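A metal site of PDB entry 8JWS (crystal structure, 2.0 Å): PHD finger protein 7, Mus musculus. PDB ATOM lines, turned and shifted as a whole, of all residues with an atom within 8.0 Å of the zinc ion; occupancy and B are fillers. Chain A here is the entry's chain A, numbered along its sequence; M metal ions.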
ATOM      1  N   PHE A  77      16.876 -21.291 -23.660  1.00  0.00           N
ATOM      2  CA  PHE A  77      16.163 -22.187 -22.764  1.00  0.00           C
ATOM      3  C   PHE A  77      15.043 -22.938 -23.492  1.00  0.00           C
ATOM      4  O   PHE A  77      14.651 -24.016 -23.051  1.00  0.00           O
ATOM      5  CB  PHE A  77      15.630 -21.453 -21.536  1.00  0.00           C
ATOM      6  CG  PHE A  77      14.332 -20.695 -21.705  1.00  0.00           C
ATOM      7  CD1 PHE A  77      13.109 -21.334 -21.517  1.00  0.00           C
ATOM      8  CD2 PHE A  77      14.333 -19.347 -22.012  1.00  0.00           C
ATOM      9  CE1 PHE A  77      11.915 -20.621 -21.685  1.00  0.00           C
ATOM     10  CE2 PHE A  77      13.133 -18.650 -22.174  1.00  0.00           C
ATOM     11  CZ  PHE A  77      11.946 -19.290 -22.006  1.00  0.00           C
ATOM     12  N   ARG A  87      18.368 -11.701 -23.177  1.00  0.00           N
ATOM     13  CA  ARG A  87      18.393 -12.117 -21.807  1.00  0.00           C
ATOM     14  C   ARG A  87      17.230 -11.527 -21.056  1.00  0.00           C
ATOM     15  O   ARG A  87      16.934 -10.356 -21.198  1.00  0.00           O
ATOM     16  CB  ARG A  87      19.714 -11.659 -21.172  1.00  0.00           C
ATOM     17  CG  ARG A  87      19.708 -11.624 -19.663  1.00  0.00           C
ATOM     18  CD  ARG A  87      20.002 -12.987 -19.075  1.00  0.00           C
ATOM     19  NE  ARG A  87      20.323 -12.901 -17.660  1.00  0.00           N
ATOM     20  CZ  ARG A  87      21.548 -12.675 -17.191  1.00  0.00           C
ATOM     21  NH1 ARG A  87      22.561 -12.516 -18.028  1.00  0.00           N
ATOM     22  NH2 ARG A  87      21.751 -12.610 -15.887  1.00  0.00           N
ATOM     23  N   CYS A  88      16.548 -12.354 -20.285  1.00  0.00           N
ATOM     24  CA  CYS A  88      15.481 -11.853 -19.420  1.00  0.00           C
ATOM     25  C   CYS A  88      16.055 -10.746 -18.536  1.00  0.00           C
ATOM     26  O   CYS A  88      17.095 -10.927 -17.910  1.00  0.00           O
ATOM     27  CB  CYS A  88      14.859 -12.944 -18.563  1.00  0.00           C
ATOM     28  SG  CYS A  88      13.588 -12.346 -17.407  1.00  0.00           S
ATOM     29  N   GLN A  89      15.352  -9.618 -18.481  1.00  0.00           N
ATOM     30  CA  GLN A  89      15.882  -8.440 -17.818  1.00  0.00           C
ATOM     31  C   GLN A  89      15.520  -8.313 -16.333  1.00  0.00           C
ATOM     32  O   GLN A  89      15.857  -7.312 -15.731  1.00  0.00           O
ATOM     33  CB  GLN A  89      15.468  -7.177 -18.600  1.00  0.00           C
ATOM     34  CG  GLN A  89      16.156  -7.104 -19.942  1.00  0.00           C
ATOM     35  CD  GLN A  89      17.668  -7.049 -19.771  1.00  0.00           C
ATOM     36  OE1 GLN A  89      18.175  -6.155 -19.080  1.00  0.00           O
ATOM     37  NE2 GLN A  89      18.401  -7.972 -20.362  1.00  0.00           N
ATOM     38  N   ASN A  90      14.985  -9.394 -15.771  1.00  0.00           N
ATOM     39  CA  ASN A  90      14.793  -9.438 -14.339  1.00  0.00           C
ATOM     40  C   ASN A  90      16.191  -9.682 -13.794  1.00  0.00           C
ATOM     41  O   ASN A  90      16.886 -10.582 -14.234  1.00  0.00           O
ATOM     42  CB  ASN A  90      13.833 -10.547 -13.927  1.00  0.00           C
ATOM     43  CG  ASN A  90      13.828 -10.784 -12.439  1.00  0.00           C
ATOM     44  OD1 ASN A  90      14.693 -11.462 -11.896  1.00  0.00           O
ATOM     45  ND2 ASN A  90      12.842 -10.212 -11.760  1.00  0.00           N
ATOM     46  N   ASP A  91      16.605  -8.885 -12.830  1.00  0.00           N
ATOM     47  CA  ASP A  91      17.957  -8.980 -12.289  1.00  0.00           C
ATOM     48  C   ASP A  91      18.389 -10.303 -11.636  1.00  0.00           C
ATOM     49  O   ASP A  91      19.561 -10.566 -11.474  1.00  0.00           O
ATOM     50  CB  ASP A  91      18.131  -7.891 -11.253  1.00  0.00           C
ATOM     51  CG  ASP A  91      17.838  -6.509 -11.826  1.00  0.00           C
ATOM     52  OD1 ASP A  91      18.260  -6.231 -12.964  1.00  0.00           O
ATOM     53  OD2 ASP A  91      17.194  -5.708 -11.131  1.00  0.00           O
ATOM     54  N   GLN A  92      17.431 -11.106 -11.237  1.00  0.00           N
ATOM     55  CA  GLN A  92      17.746 -12.386 -10.637  1.00  0.00           C
ATOM     56  C   GLN A  92      17.307 -13.532 -11.538  1.00  0.00           C
ATOM     57  O   GLN A  92      16.879 -14.559 -11.053  1.00  0.00           O
ATOM     58  CB  GLN A  92      17.148 -12.458  -9.241  1.00  0.00           C
ATOM     59  CG  GLN A  92      17.757 -11.469  -8.274  1.00  0.00           C
ATOM     60  CD  GLN A  92      17.122 -10.109  -8.363  1.00  0.00           C
ATOM     61  OE1 GLN A  92      15.989  -9.972  -8.796  1.00  0.00           O
ATOM     62  NE2 GLN A  92      17.864  -9.084  -7.974  1.00  0.00           N
ATOM     63  N   CYS A  93      17.407 -13.347 -12.843  1.00  0.00           N
ATOM     64  CA  CYS A  93      17.075 -14.346 -13.837  1.00  0.00           C
ATOM     65  C   CYS A  93      18.229 -14.501 -14.826  1.00  0.00           C
ATOM     66  O   CYS A  93      18.798 -13.516 -15.268  1.00  0.00           O
ATOM     67  CB  CYS A  93      15.799 -13.985 -14.597  1.00  0.00           C
ATOM     68  SG  CYS A  93      15.190 -15.293 -15.710  1.00  0.00           S
ATOM     69  N   VAL A  94      18.504 -15.762 -15.195  1.00  0.00           N
ATOM     70  CA  VAL A  94      19.595 -16.087 -16.106  1.00  0.00           C
ATOM     71  C   VAL A  94      19.104 -16.720 -17.400  1.00  0.00           C
ATOM     72  O   VAL A  94      19.919 -17.239 -18.172  1.00  0.00           O
ATOM     73  CB  VAL A  94      20.633 -17.011 -15.407  1.00  0.00           C
ATOM     74  CG1 VAL A  94      21.309 -16.313 -14.236  1.00  0.00           C
ATOM     75  CG2 VAL A  94      20.028 -18.343 -14.975  1.00  0.00           C
ATOM     76  N   GLN A  95      17.787 -16.693 -17.659  1.00  0.00           N
ATOM     77  CA  GLN A  95      17.248 -17.253 -18.883  1.00  0.00           C
ATOM     78  C   GLN A  95      17.649 -16.399 -20.088  1.00  0.00           C
ATOM     79  O   GLN A  95      17.502 -15.163 -20.065  1.00  0.00           O
ATOM     80  CB  GLN A  95      15.708 -17.327 -18.853  1.00  0.00           C
ATOM     81  CG  GLN A  95      15.138 -18.213 -17.754  1.00  0.00           C
ATOM     82  CD  GLN A  95      15.340 -19.663 -18.070  1.00  0.00           C
ATOM     83  OE1 GLN A  95      16.455 -20.191 -18.010  1.00  0.00           O
ATOM     84  NE2 GLN A  95      14.250 -20.373 -18.384  1.00  0.00           N
ATOM     85  N   ASN A  96      18.161 -17.055 -21.129  1.00  0.00           N
ATOM     86  CA  ASN A  96      18.463 -16.425 -22.405  1.00  0.00           C
ATOM     87  C   ASN A  96      17.665 -17.140 -23.490  1.00  0.00           C
ATOM     88  O   ASN A  96      17.332 -18.311 -23.330  1.00  0.00           O
ATOM     89  CB  ASN A  96      19.930 -16.477 -22.760  1.00  0.00           C
ATOM     90  CG  ASN A  96      20.822 -15.777 -21.770  1.00  0.00           C
ATOM     91  OD1 ASN A  96      21.183 -14.634 -21.988  1.00  0.00           O
ATOM     92  ND2 ASN A  96      21.178 -16.426 -20.693  1.00  0.00           N
ATOM     93  N   PHE A  97      17.359 -16.422 -24.579  1.00  0.00           N
ATOM     94  CA  PHE A  97      16.579 -17.018 -25.663  1.00  0.00           C
ATOM     95  C   PHE A  97      16.767 -16.300 -26.990  1.00  0.00           C
ATOM     96  O   PHE A  97      17.166 -15.143 -27.028  1.00  0.00           O
ATOM     97  CB  PHE A  97      15.087 -17.050 -25.279  1.00  0.00           C
ATOM     98  CG  PHE A  97      14.504 -15.771 -24.747  1.00  0.00           C
ATOM     99  CD1 PHE A  97      14.621 -15.443 -23.396  1.00  0.00           C
ATOM    100  CD2 PHE A  97      13.844 -14.887 -25.583  1.00  0.00           C
ATOM    101  CE1 PHE A  97      14.051 -14.270 -22.902  1.00  0.00           C
ATOM    102  CE2 PHE A  97      13.293 -13.708 -25.086  1.00  0.00           C
ATOM    103  CZ  PHE A  97      13.393 -13.415 -23.755  1.00  0.00           C
ATOM    104  N   CYS A 107       7.339 -15.106 -23.709  1.00  0.00           N
ATOM    105  CA  CYS A 107       8.254 -14.051 -23.328  1.00  0.00           C
ATOM    106  C   CYS A 107       7.707 -12.708 -23.813  1.00  0.00           C
ATOM    107  O   CYS A 107       7.057 -12.653 -24.836  1.00  0.00           O
ATOM    108  CB  CYS A 107       9.661 -14.300 -23.882  1.00  0.00           C
ATOM    109  SG  CYS A 107      10.439 -15.775 -23.199  1.00  0.00           S
ATOM    110  N   SER A 117      13.370  -7.320 -22.582  1.00  0.00           N
ATOM    111  CA  SER A 117      12.525  -8.500 -22.704  1.00  0.00           C
ATOM    112  C   SER A 117      12.518  -9.263 -21.385  1.00  0.00           C
ATOM    113  O   SER A 117      13.461  -9.133 -20.607  1.00  0.00           O
ATOM    114  CB  SER A 117      13.013  -9.398 -23.841  1.00  0.00           C
ATOM    115  OG  SER A 117      12.889  -8.760 -25.103  1.00  0.00           O
ATOM    116  N   TYR A 118      11.468 -10.042 -21.189  1.00  0.00           N
ATOM    117  CA  TYR A 118      11.284 -10.820 -19.970  1.00  0.00           C
ATOM    118  C   TYR A 118      10.767 -12.216 -20.236  1.00  0.00           C
ATOM    119  O   TYR A 118       9.988 -12.420 -21.154  1.00  0.00           O
ATOM    120  CB  TYR A 118      10.300 -10.116 -19.019  1.00  0.00           C
ATOM    121  CG  TYR A 118      10.751  -8.758 -18.538  1.00  0.00           C
ATOM    122  CD1 TYR A 118      11.550  -8.640 -17.424  1.00  0.00           C
ATOM    123  CD2 TYR A 118      10.373  -7.599 -19.202  1.00  0.00           C
ATOM    124  CE1 TYR A 118      11.968  -7.410 -16.977  1.00  0.00           C
ATOM    125  CE2 TYR A 118      10.778  -6.361 -18.763  1.00  0.00           C
ATOM    126  CZ  TYR A 118      11.575  -6.267 -17.646  1.00  0.00           C
ATOM    127  OH  TYR A 118      11.988  -5.052 -17.192  1.00  0.00           O
ATOM    128  N   CYS A 119      11.202 -13.171 -19.445  1.00  0.00           N
ATOM    129  CA  CYS A 119      10.651 -14.493 -19.577  1.00  0.00           C
ATOM    130  C   CYS A 119       9.217 -14.416 -19.049  1.00  0.00           C
ATOM    131  O   CYS A 119       8.823 -13.411 -18.482  1.00  0.00           O
ATOM    132  CB  CYS A 119      11.529 -15.518 -18.836  1.00  0.00           C
ATOM    133  SG  CYS A 119      11.228 -15.691 -17.078  1.00  0.00           S
ATOM    134  N   ARG A 120       8.446 -15.459 -19.237  1.00  0.00           N
ATOM    135  CA  ARG A 120       7.052 -15.443 -18.839  1.00  0.00           C
ATOM    136  C   ARG A 120       6.866 -15.248 -17.332  1.00  0.00           C
ATOM    137  O   ARG A 120       5.957 -14.567 -16.913  1.00  0.00           O
ATOM    138  CB  ARG A 120       6.366 -16.726 -19.305  1.00  0.00           C
ATOM    139  CG  ARG A 120       4.850 -16.662 -19.383  1.00  0.00           C
ATOM    140  CD  ARG A 120       4.306 -18.006 -19.852  1.00  0.00           C
ATOM    141  NE  ARG A 120       2.949 -18.250 -19.376  1.00  0.00           N
ATOM    142  CZ  ARG A 120       2.584 -19.334 -18.698  1.00  0.00           C
ATOM    143  NH1 ARG A 120       3.473 -20.271 -18.409  1.00  0.00           N
ATOM    144  NH2 ARG A 120       1.329 -19.480 -18.308  1.00  0.00           N
ATOM    145  N   LYS A 121       7.754 -15.818 -16.523  1.00  0.00           N
ATOM    146  CA  LYS A 121       7.636 -15.722 -15.083  1.00  0.00           C
ATOM    147  C   LYS A 121       7.990 -14.342 -14.587  1.00  0.00           C
ATOM    148  O   LYS A 121       7.654 -13.999 -13.469  1.00  0.00           O
ATOM    149  CB  LYS A 121       8.498 -16.771 -14.400  1.00  0.00           C
ATOM    150  CG  LYS A 121       9.920 -16.333 -14.089  1.00  0.00           C
ATOM    151  CD  LYS A 121      10.625 -17.326 -13.188  1.00  0.00           C
ATOM    152  CE  LYS A 121       9.788 -17.645 -11.955  1.00  0.00           C
ATOM    153  NZ  LYS A 121      10.229 -18.910 -11.297  1.00  0.00           N
ATOM    154  N   HIS A 122       8.628 -13.547 -15.429  1.00  0.00           N
ATOM    155  CA  HIS A 122       9.084 -12.238 -15.012  1.00  0.00           C
ATOM    156  C   HIS A 122       8.423 -11.091 -15.789  1.00  0.00           C
ATOM    157  O   HIS A 122       8.920  -9.981 -15.785  1.00  0.00           O
ATOM    158  CB  HIS A 122      10.608 -12.205 -15.126  1.00  0.00           C
ATOM    159  CG  HIS A 122      11.313 -13.085 -14.144  1.00  0.00           C
ATOM    160  ND1 HIS A 122      12.296 -13.974 -14.502  1.00  0.00           N
ATOM    161  CD2 HIS A 122      11.169 -13.198 -12.801  1.00  0.00           C
ATOM    162  CE1 HIS A 122      12.730 -14.601 -13.427  1.00  0.00           C
ATOM    163  NE2 HIS A 122      12.071 -14.152 -12.382  1.00  0.00           N
ATOM    164  N   ARG A 123       7.288 -11.356 -16.441  1.00  0.00           N
ATOM    165  CA  ARG A 123       6.562 -10.296 -17.118  1.00  0.00           C
ATOM    166  C   ARG A 123       6.164  -9.227 -16.110  1.00  0.00           C
ATOM    167  O   ARG A 123       5.559  -9.548 -15.101  1.00  0.00           O
ATOM    168  CB  ARG A 123       5.314 -10.857 -17.841  1.00  0.00           C
ATOM    169  CG  ARG A 123       5.684 -11.607 -19.096  1.00  0.00           C
ATOM    170  CD  ARG A 123       4.745 -12.733 -19.413  1.00  0.00           C
ATOM    171  NE  ARG A 123       3.434 -12.293 -19.884  1.00  0.00           N
ATOM    172  CZ  ARG A 123       2.700 -12.993 -20.746  1.00  0.00           C
ATOM    173  NH1 ARG A 123       3.179 -14.064 -21.350  1.00  0.00           N
ATOM    174  NH2 ARG A 123       1.438 -12.617 -20.973  1.00  0.00           N
HETATM  175 ZN    ZN M   1      13.120 -14.316 -16.261  1.00  0.00          ZN
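The backbone NH (N) of Asn 90 sits close to the side-chain sulfur (SG) of Cys 88.
The backbone NH of Cys 88 is in hydrogen-bond range of the backbone carbonyl oxygen of Gln 95, 3.0 Å away.
The side-chain amide oxygen of Asn 90 sits at hydrogen-bond distance from the backbone NH of Cys 93 (3.4 Å).
N of Gln 95 lies close to SG of Cys 93 (3.5 Å).
The backbone carbonyl oxygen (O) of Cys 93 is in hydrogen-bond range of the guanidinium group (NE) of Arg 87, at 2.9 Å.
The backbone NH (N) of Lys 121 lies close to the side-chain sulfur (SG) of Cys 119.
Four residues have an atom within 4 Å of the zinc ion: Cys 88, Cys 93, Cys 119 and His 122.
The nearest printed residue that does not touch the zinc ion is Lys 121 (4.4 Å).
The zinc ion is bound by a ring nitrogen (ND1) of His 122, the side-chain sulfur (SG) of Cys 88, the side-chain sulfur (SG) of Cys 93 and the side-chain sulfur (SG) of Cys 119.
The zinc ion has four donor atoms within binding distance.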
